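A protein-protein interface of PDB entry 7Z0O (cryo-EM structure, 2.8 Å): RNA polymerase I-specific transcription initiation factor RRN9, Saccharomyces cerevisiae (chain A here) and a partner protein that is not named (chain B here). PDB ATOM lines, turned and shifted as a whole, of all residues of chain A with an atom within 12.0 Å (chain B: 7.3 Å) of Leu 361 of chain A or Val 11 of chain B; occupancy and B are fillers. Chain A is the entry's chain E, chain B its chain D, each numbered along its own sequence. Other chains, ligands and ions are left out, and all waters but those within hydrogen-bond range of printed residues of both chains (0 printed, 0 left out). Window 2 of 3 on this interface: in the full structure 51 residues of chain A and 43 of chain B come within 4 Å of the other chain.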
ATOM      1  N   LEU A 354     -21.613  10.496  -7.974  1.00  0.00           N
ATOM      2  CA  LEU A 354     -21.735  10.554  -6.522  1.00  0.00           C
ATOM      3  C   LEU A 354     -22.801  11.555  -6.095  1.00  0.00           C
ATOM      4  O   LEU A 354     -23.531  11.319  -5.126  1.00  0.00           O
ATOM      5  CB  LEU A 354     -20.373  10.900  -5.913  1.00  0.00           C
ATOM      6  CG  LEU A 354     -20.060  10.750  -4.419  1.00  0.00           C
ATOM      7  CD1 LEU A 354     -20.723  11.815  -3.567  1.00  0.00           C
ATOM      8  CD2 LEU A 354     -20.458   9.372  -3.936  1.00  0.00           C
ATOM      9  N   ASP A 355     -22.908  12.678  -6.810  1.00  0.00           N
ATOM     10  CA  ASP A 355     -23.845  13.725  -6.413  1.00  0.00           C
ATOM     11  C   ASP A 355     -25.294  13.260  -6.498  1.00  0.00           C
ATOM     12  O   ASP A 355     -26.153  13.771  -5.771  1.00  0.00           O
ATOM     13  CB  ASP A 355     -23.640  14.965  -7.280  1.00  0.00           C
ATOM     14  CG  ASP A 355     -24.217  16.217  -6.652  1.00  0.00           C
ATOM     15  OD1 ASP A 355     -24.670  16.146  -5.490  1.00  0.00           O
ATOM     16  OD2 ASP A 355     -24.223  17.272  -7.321  1.00  0.00           O
ATOM     17  N   CYS A 357     -26.503  10.445  -5.572  1.00  0.00           N
ATOM     18  CA  CYS A 357     -26.819   9.417  -4.588  1.00  0.00           C
ATOM     19  C   CYS A 357     -26.886   9.923  -3.156  1.00  0.00           C
ATOM     20  O   CYS A 357     -27.531   9.282  -2.325  1.00  0.00           O
ATOM     21  CB  CYS A 357     -25.790   8.282  -4.660  1.00  0.00           C
ATOM     22  SG  CYS A 357     -25.566   7.586  -6.309  1.00  0.00           S
ATOM     23  N   LEU A 358     -26.245  11.046  -2.842  1.00  0.00           N
ATOM     24  CA  LEU A 358     -26.213  11.523  -1.465  1.00  0.00           C
ATOM     25  C   LEU A 358     -27.587  12.001  -1.020  1.00  0.00           C
ATOM     26  O   LEU A 358     -28.444  12.337  -1.840  1.00  0.00           O
ATOM     27  CB  LEU A 358     -25.199  12.653  -1.314  1.00  0.00           C
ATOM     28  CG  LEU A 358     -23.737  12.313  -1.585  1.00  0.00           C
ATOM     29  CD1 LEU A 358     -22.851  13.462  -1.144  1.00  0.00           C
ATOM     30  CD2 LEU A 358     -23.344  11.029  -0.881  1.00  0.00           C
ATOM     31  N   ILE A 359     -27.792  12.029   0.292  1.00  0.00           N
ATOM     32  CA  ILE A 359     -29.052  12.465   0.879  1.00  0.00           C
ATOM     33  C   ILE A 359     -28.808  13.727   1.693  1.00  0.00           C
ATOM     34  O   ILE A 359     -27.859  13.797   2.482  1.00  0.00           O
ATOM     35  CB  ILE A 359     -29.666  11.360   1.752  1.00  0.00           C
ATOM     36  CG1 ILE A 359     -30.125  10.189   0.889  1.00  0.00           C
ATOM     37  CG2 ILE A 359     -30.828  11.901   2.561  1.00  0.00           C
ATOM     38  CD1 ILE A 359     -30.490   8.969   1.688  1.00  0.00           C
ATOM     39  N   GLU A 360     -29.657  14.729   1.493  1.00  0.00           N
ATOM     40  CA  GLU A 360     -29.653  15.944   2.291  1.00  0.00           C
ATOM     41  C   GLU A 360     -31.020  16.119   2.937  1.00  0.00           C
ATOM     42  O   GLU A 360     -32.052  15.866   2.307  1.00  0.00           O
ATOM     43  CB  GLU A 360     -29.299  17.168   1.439  1.00  0.00           C
ATOM     44  CG  GLU A 360     -30.256  17.432   0.289  1.00  0.00           C
ATOM     45  CD  GLU A 360     -29.872  16.686  -0.974  1.00  0.00           C
ATOM     46  OE1 GLU A 360     -29.018  15.777  -0.894  1.00  0.00           O
ATOM     47  OE2 GLU A 360     -30.423  17.008  -2.047  1.00  0.00           O
ATOM     48  N   LEU A 361     -31.025  16.535   4.197  1.00  0.00           N
ATOM     49  CA  LEU A 361     -32.273  16.682   4.938  1.00  0.00           C
ATOM     50  C   LEU A 361     -32.578  18.145   5.236  1.00  0.00           C
ATOM     51  O   LEU A 361     -33.709  18.493   5.574  1.00  0.00           O
ATOM     52  CB  LEU A 361     -32.217  15.881   6.238  1.00  0.00           C
ATOM     53  CG  LEU A 361     -32.076  14.367   6.081  1.00  0.00           C
ATOM     54  CD1 LEU A 361     -32.041  13.686   7.439  1.00  0.00           C
ATOM     55  CD2 LEU A 361     -33.201  13.808   5.225  1.00  0.00           C
ATOM     56  N   GLN B   5     -33.616   8.894  17.243  1.00  0.00           N
ATOM     57  CA  GLN B   5     -32.943   9.603  16.162  1.00  0.00           C
ATOM     58  C   GLN B   5     -32.311   8.637  15.169  1.00  0.00           C
ATOM     59  O   GLN B   5     -31.270   8.940  14.578  1.00  0.00           O
ATOM     60  CB  GLN B   5     -31.893  10.571  16.712  1.00  0.00           C
ATOM     61  CG  GLN B   5     -30.797   9.917  17.531  1.00  0.00           C
ATOM     62  CD  GLN B   5     -29.710  10.896  17.920  1.00  0.00           C
ATOM     63  OE1 GLN B   5     -29.581  11.966  17.325  1.00  0.00           O
ATOM     64  NE2 GLN B   5     -28.918  10.536  18.924  1.00  0.00           N
ATOM     65  N   GLN B   6     -32.931   7.470  14.970  1.00  0.00           N
ATOM     66  CA  GLN B   6     -32.381   6.485  14.044  1.00  0.00           C
ATOM     67  C   GLN B   6     -32.346   7.011  12.617  1.00  0.00           C
ATOM     68  O   GLN B   6     -31.505   6.580  11.819  1.00  0.00           O
ATOM     69  CB  GLN B   6     -33.201   5.199  14.097  1.00  0.00           C
ATOM     70  CG  GLN B   6     -33.899   4.964  15.417  1.00  0.00           C
ATOM     71  CD  GLN B   6     -35.110   4.071  15.272  1.00  0.00           C
ATOM     72  OE1 GLN B   6     -35.287   3.407  14.250  1.00  0.00           O
ATOM     73  NE2 GLN B   6     -35.958   4.053  16.291  1.00  0.00           N
ATOM     74  N   LEU B   7     -33.251   7.929  12.276  1.00  0.00           N
ATOM     75  CA  LEU B   7     -33.337   8.413  10.902  1.00  0.00           C
ATOM     76  C   LEU B   7     -32.053   9.123  10.494  1.00  0.00           C
ATOM     77  O   LEU B   7     -31.508   8.870   9.415  1.00  0.00           O
ATOM     78  CB  LEU B   7     -34.549   9.336  10.756  1.00  0.00           C
ATOM     79  CG  LEU B   7     -35.153   9.587   9.370  1.00  0.00           C
ATOM     80  CD1 LEU B   7     -34.281  10.471   8.489  1.00  0.00           C
ATOM     81  CD2 LEU B   7     -35.436   8.263   8.682  1.00  0.00           C
ATOM     82  N   ARG B   8     -31.549  10.014  11.350  1.00  0.00           N
ATOM     83  CA  ARG B   8     -30.320  10.726  11.016  1.00  0.00           C
ATOM     84  C   ARG B   8     -29.116   9.794  11.062  1.00  0.00           C
ATOM     85  O   ARG B   8     -28.199   9.920  10.245  1.00  0.00           O
ATOM     86  CB  ARG B   8     -30.126  11.925  11.947  1.00  0.00           C
ATOM     87  CG  ARG B   8     -29.755  11.579  13.377  1.00  0.00           C
ATOM     88  CD  ARG B   8     -28.865  12.645  13.989  1.00  0.00           C
ATOM     89  NE  ARG B   8     -27.451  12.321  13.851  1.00  0.00           N
ATOM     90  CZ  ARG B   8     -26.764  11.578  14.708  1.00  0.00           C
ATOM     91  NH1 ARG B   8     -27.334  11.053  15.780  1.00  0.00           N
ATOM     92  NH2 ARG B   8     -25.472  11.356  14.484  1.00  0.00           N
ATOM     93  N   LYS B   9     -29.108   8.843  12.000  1.00  0.00           N
ATOM     94  CA  LYS B   9     -28.002   7.894  12.081  1.00  0.00           C
ATOM     95  C   LYS B   9     -27.931   7.029  10.831  1.00  0.00           C
ATOM     96  O   LYS B   9     -26.839   6.725  10.337  1.00  0.00           O
ATOM     97  CB  LYS B   9     -28.147   7.024  13.327  1.00  0.00           C
ATOM     98  CG  LYS B   9     -27.859   7.751  14.625  1.00  0.00           C
ATOM     99  CD  LYS B   9     -28.138   6.864  15.823  1.00  0.00           C
ATOM    100  CE  LYS B   9     -27.642   7.505  17.104  1.00  0.00           C
ATOM    101  NZ  LYS B   9     -27.259   6.488  18.116  1.00  0.00           N
ATOM    102  N   TYR B  10     -29.086   6.616  10.310  1.00  0.00           N
ATOM    103  CA  TYR B  10     -29.109   5.841   9.075  1.00  0.00           C
ATOM    104  C   TYR B  10     -28.605   6.664   7.897  1.00  0.00           C
ATOM    105  O   TYR B  10     -27.930   6.137   7.006  1.00  0.00           O
ATOM    106  CB  TYR B  10     -30.523   5.328   8.811  1.00  0.00           C
ATOM    107  CG  TYR B  10     -30.666   4.540   7.530  1.00  0.00           C
ATOM    108  CD1 TYR B  10     -30.398   3.181   7.498  1.00  0.00           C
ATOM    109  CD2 TYR B  10     -31.073   5.156   6.355  1.00  0.00           C
ATOM    110  CE1 TYR B  10     -30.528   2.459   6.333  1.00  0.00           C
ATOM    111  CE2 TYR B  10     -31.204   4.442   5.187  1.00  0.00           C
ATOM    112  CZ  TYR B  10     -30.931   3.094   5.181  1.00  0.00           C
ATOM    113  OH  TYR B  10     -31.061   2.379   4.016  1.00  0.00           O
ATOM    114  N   VAL B  11     -28.928   7.959   7.873  1.00  0.00           N
ATOM    115  CA  VAL B  11     -28.568   8.796   6.733  1.00  0.00           C
ATOM    116  C   VAL B  11     -27.054   8.930   6.611  1.00  0.00           C
ATOM    117  O   VAL B  11     -26.497   8.803   5.514  1.00  0.00           O
ATOM    118  CB  VAL B  11     -29.255  10.168   6.845  1.00  0.00           C
ATOM    119  CG1 VAL B  11     -28.562  11.187   5.961  1.00  0.00           C
ATOM    120  CG2 VAL B  11     -30.718  10.049   6.469  1.00  0.00           C
ATOM    121  N   GLU B  12     -26.361   9.185   7.724  1.00  0.00           N
ATOM    122  CA  GLU B  12     -24.904   9.265   7.668  1.00  0.00           C
ATOM    123  C   GLU B  12     -24.291   7.921   7.304  1.00  0.00           C
ATOM    124  O   GLU B  12     -23.295   7.867   6.576  1.00  0.00           O
ATOM    125  CB  GLU B  12     -24.332   9.768   8.992  1.00  0.00           C
ATOM    126  CG  GLU B  12     -25.286  10.589   9.826  1.00  0.00           C
ATOM    127  CD  GLU B  12     -24.570  11.472  10.828  1.00  0.00           C
ATOM    128  OE1 GLU B  12     -24.856  12.687  10.864  1.00  0.00           O
ATOM    129  OE2 GLU B  12     -23.720  10.951  11.580  1.00  0.00           O
ATOM    130  N   LEU B  13     -24.865   6.827   7.806  1.00  0.00           N
ATOM    131  CA  LEU B  13     -24.375   5.505   7.434  1.00  0.00           C
ATOM    132  C   LEU B  13     -24.514   5.280   5.935  1.00  0.00           C
ATOM    133  O   LEU B  13     -23.596   4.770   5.283  1.00  0.00           O
ATOM    134  CB  LEU B  13     -25.126   4.428   8.214  1.00  0.00           C
ATOM    135  CG  LEU B  13     -24.935   2.988   7.736  1.00  0.00           C
ATOM    136  CD1 LEU B  13     -23.500   2.540   7.944  1.00  0.00           C
ATOM    137  CD2 LEU B  13     -25.897   2.057   8.449  1.00  0.00           C
ATOM    138  N   TYR B  14     -25.659   5.662   5.369  1.00  0.00           N
ATOM    139  CA  TYR B  14     -25.849   5.537   3.929  1.00  0.00           C
ATOM    140  C   TYR B  14     -24.900   6.450   3.163  1.00  0.00           C
ATOM    141  O   TYR B  14     -24.302   6.034   2.164  1.00  0.00           O
ATOM    142  CB  TYR B  14     -27.300   5.846   3.567  1.00  0.00           C
ATOM    143  CG  TYR B  14     -27.549   5.976   2.083  1.00  0.00           C
ATOM    144  CD1 TYR B  14     -27.791   4.860   1.300  1.00  0.00           C
ATOM    145  CD2 TYR B  14     -27.543   7.218   1.466  1.00  0.00           C
ATOM    146  CE1 TYR B  14     -28.019   4.977  -0.053  1.00  0.00           C
ATOM    147  CE2 TYR B  14     -27.768   7.343   0.116  1.00  0.00           C
ATOM    148  CZ  TYR B  14     -28.006   6.221  -0.638  1.00  0.00           C
ATOM    149  OH  TYR B  14     -28.232   6.344  -1.987  1.00  0.00           O
ATOM    150  N   ASN B  15     -24.755   7.699   3.610  1.00  0.00           N
ATOM    151  CA  ASN B  15     -23.907   8.647   2.893  1.00  0.00           C
ATOM    152  C   ASN B  15     -22.446   8.220   2.918  1.00  0.00           C
ATOM    153  O   ASN B  15     -21.746   8.317   1.905  1.00  0.00           O
ATOM    154  CB  ASN B  15     -24.062  10.046   3.485  1.00  0.00           C
ATOM    155  CG  ASN B  15     -25.302  10.754   2.987  1.00  0.00           C
ATOM    156  OD1 ASN B  15     -25.681  10.625   1.826  1.00  0.00           O
ATOM    157  ND2 ASN B  15     -25.938  11.515   3.865  1.00  0.00           N
ATOM    158  N   LYS B  16     -21.964   7.754   4.071  1.00  0.00           N
ATOM    159  CA  LYS B  16     -20.575   7.317   4.163  1.00  0.00           C
ATOM    160  C   LYS B  16     -20.335   6.068   3.328  1.00  0.00           C
ATOM    161  O   LYS B  16     -19.268   5.911   2.724  1.00  0.00           O
ATOM    162  CB  LYS B  16     -20.201   7.073   5.623  1.00  0.00           C
ATOM    163  CG  LYS B  16     -20.131   8.338   6.454  1.00  0.00           C
ATOM    164  CD  LYS B  16     -19.932   8.022   7.922  1.00  0.00           C
ATOM    165  CE  LYS B  16     -20.095   9.265   8.776  1.00  0.00           C
ATOM    166  NZ  LYS B  16     -19.035  10.270   8.498  1.00  0.00           N
ATOM    167  N   GLU B  17     -21.312   5.160   3.290  1.00  0.00           N
ATOM    168  CA  GLU B  17     -21.178   3.962   2.468  1.00  0.00           C
ATOM    169  C   GLU B  17     -21.141   4.306   0.986  1.00  0.00           C
ATOM    170  O   GLU B  17     -20.377   3.709   0.220  1.00  0.00           O
ATOM    171  CB  GLU B  17     -22.323   2.998   2.762  1.00  0.00           C
ATOM    172  CG  GLU B  17     -22.115   2.159   4.001  1.00  0.00           C
ATOM    173  CD  GLU B  17     -22.752   0.795   3.887  1.00  0.00           C
ATOM    174  OE1 GLU B  17     -22.920   0.306   2.749  1.00  0.00           O
ATOM    175  OE2 GLU B  17     -23.092   0.212   4.936  1.00  0.00           O
ATOM    176  N   LEU B 139     -36.730   2.253   7.148  1.00  0.00           N
ATOM    177  CA  LEU B 139     -35.877   3.433   7.233  1.00  0.00           C
ATOM    178  C   LEU B 139     -35.670   4.069   5.865  1.00  0.00           C
ATOM    179  O   LEU B 139     -35.716   5.297   5.730  1.00  0.00           O
ATOM    180  CB  LEU B 139     -34.535   3.065   7.861  1.00  0.00           C
ATOM    181  CG  LEU B 139     -34.425   3.229   9.376  1.00  0.00           C
ATOM    182  CD1 LEU B 139     -33.151   2.589   9.891  1.00  0.00           C
ATOM    183  CD2 LEU B 139     -34.473   4.697   9.752  1.00  0.00           C
ATOM    184  N   THR B 142     -38.913   5.775   4.736  1.00  0.00           N
ATOM    185  CA  THR B 142     -39.105   7.017   5.475  1.00  0.00           C
ATOM    186  C   THR B 142     -38.221   8.126   4.921  1.00  0.00           C
ATOM    187  O   THR B 142     -38.664   9.271   4.782  1.00  0.00           O
ATOM    188  CB  THR B 142     -38.817   6.795   6.958  1.00  0.00           C
ATOM    189  OG1 THR B 142     -39.646   5.736   7.452  1.00  0.00           O
ATOM    190  CG2 THR B 142     -39.098   8.059   7.748  1.00  0.00           C
ATOM    191  N   VAL B 143     -36.971   7.802   4.589  1.00  0.00           N
ATOM    192  CA  VAL B 143     -36.046   8.810   4.080  1.00  0.00           C
ATOM    193  C   VAL B 143     -36.545   9.380   2.759  1.00  0.00           C
ATOM    194  O   VAL B 143     -36.507  10.597   2.537  1.00  0.00           O
ATOM    195  CB  VAL B 143     -34.634   8.214   3.942  1.00  0.00           C
ATOM    196  CG1 VAL B 143     -33.822   9.004   2.939  1.00  0.00           C
ATOM    197  CG2 VAL B 143     -33.939   8.196   5.289  1.00  0.00           C
ATOM    198  N   ILE B 146     -39.276  12.182   3.228  1.00  0.00           N
ATOM    199  CA  ILE B 146     -38.822  13.532   3.548  1.00  0.00           C
ATOM    200  C   ILE B 146     -38.133  14.167   2.348  1.00  0.00           C
ATOM    201  O   ILE B 146     -38.383  15.332   2.015  1.00  0.00           O
ATOM    202  CB  ILE B 146     -37.900  13.516   4.781  1.00  0.00           C
ATOM    203  CG1 ILE B 146     -38.661  13.042   6.020  1.00  0.00           C
ATOM    204  CG2 ILE B 146     -37.302  14.892   5.019  1.00  0.00           C
ATOM    205  CD1 ILE B 146     -38.141  11.753   6.601  1.00  0.00           C
ATOM    206  N   THR B 147     -37.262  13.417   1.677  1.00  0.00           N
ATOM    207  CA  THR B 147     -36.500  13.951   0.557  1.00  0.00           C
ATOM    208  C   THR B 147     -37.345  14.153  -0.696  1.00  0.00           C
ATOM    209  O   THR B 147     -36.865  14.765  -1.656  1.00  0.00           O
ATOM    210  CB  THR B 147     -35.320  13.026   0.248  1.00  0.00           C
ATOM    211  OG1 THR B 147     -34.824  12.471   1.472  1.00  0.00           O
ATOM    212  CG2 THR B 147     -34.194  13.795  -0.424  1.00  0.00           C
ATOM    213  N   LEU B 362     -27.927   2.140  16.506  1.00  0.00           N
ATOM    214  CA  LEU B 362     -29.175   2.842  16.230  1.00  0.00           C
ATOM    215  C   LEU B 362     -30.053   2.946  17.470  1.00  0.00           C
ATOM    216  O   LEU B 362     -30.749   3.949  17.651  1.00  0.00           O
ATOM    217  CB  LEU B 362     -29.935   2.144  15.104  1.00  0.00           C
ATOM    218  CG  LEU B 362     -29.218   2.035  13.759  1.00  0.00           C
ATOM    219  CD1 LEU B 362     -30.046   1.223  12.780  1.00  0.00           C
ATOM    220  CD2 LEU B 362     -28.931   3.412  13.200  1.00  0.00           C
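Of the 19 printed residues of chain B, 4 touch a printed residue of chain A.
Printed residues of chain B that touch a printed residue of chain A: Val 11, Tyr 14, Asn 15 and Val 143.
Along chain B the printed residues that touch a printed residue of chain A span positions 11 to 143.
Hydrophobic or aromatic side chains of chain A that line the printed part of chain B: Leu 358, Ile 359 and Leu 361.
Among the printed residues, 6 pairs touch across the chains.
The side-chain hydroxyl (OH) of Tyr 14 of chain B lies within hydrogen-bond range of the backbone carbonyl oxygen (O) of Cys 357 of chain A, 3.0 Å away.
OD1 of Asn 15 of chain B sits at hydrogen-bond distance from N of Ile 359 of chain A, 3.0 Å away.
Among the printed residues, pairs that only touch across the chains: Leu 358 of chain A with Asn 15 of chain B (3.5 Å), Ile 359 of chain A with Tyr 14 of chain B (3.4 Å), Ile 359 of chain A with Val 143 of chain B (3.6 Å) and Leu 361 of chain A with Val 11 of chain B (3.99 Å).
The side-chain hydroxyl (OG1) of Thr 147 of chain B sits at hydrogen-bond distance from the backbone carbonyl oxygen (O) of Val 143 of chain B (2.7 Å).
The backbone carbonyl oxygen of Val 11 of chain B is in hydrogen-bond range of the side-chain amide nitrogen of Asn 15 of chain B (3.2 Å).
Of the printed residues of chain B, Cys 357 of chain A touches Tyr 14 (3.0 Å).
Printed residues of chain B within 4 Å of Leu 358 of chain A: Asn 15.
Printed residues of chain B within 4 Å of Ile 359 of chain A: Tyr 14 (3.4 Å), Asn 15 (3.0 Å) and Val 143 (3.6 Å).
Of the printed residues of chain B, Leu 361 of chain A touches Val 11 (3.99 Å).
No residue of chain A comes within 4 Å of Tyr 10 of chain B.
Printed residues of chain A within 4 Å of Val 11 of chain B: Leu 361.
No residue of chain A comes within 4 Å of Glu 12 of chain B.
No residue of chain A comes within 4 Å of Leu 13 of chain B.
Of the printed residues of chain A, Tyr 14 of chain B touches Cys 357 (3.0 Å) and Ile 359 (3.4 Å).
Val 143 of chain B touches just one residue of chain A: Ile 359.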
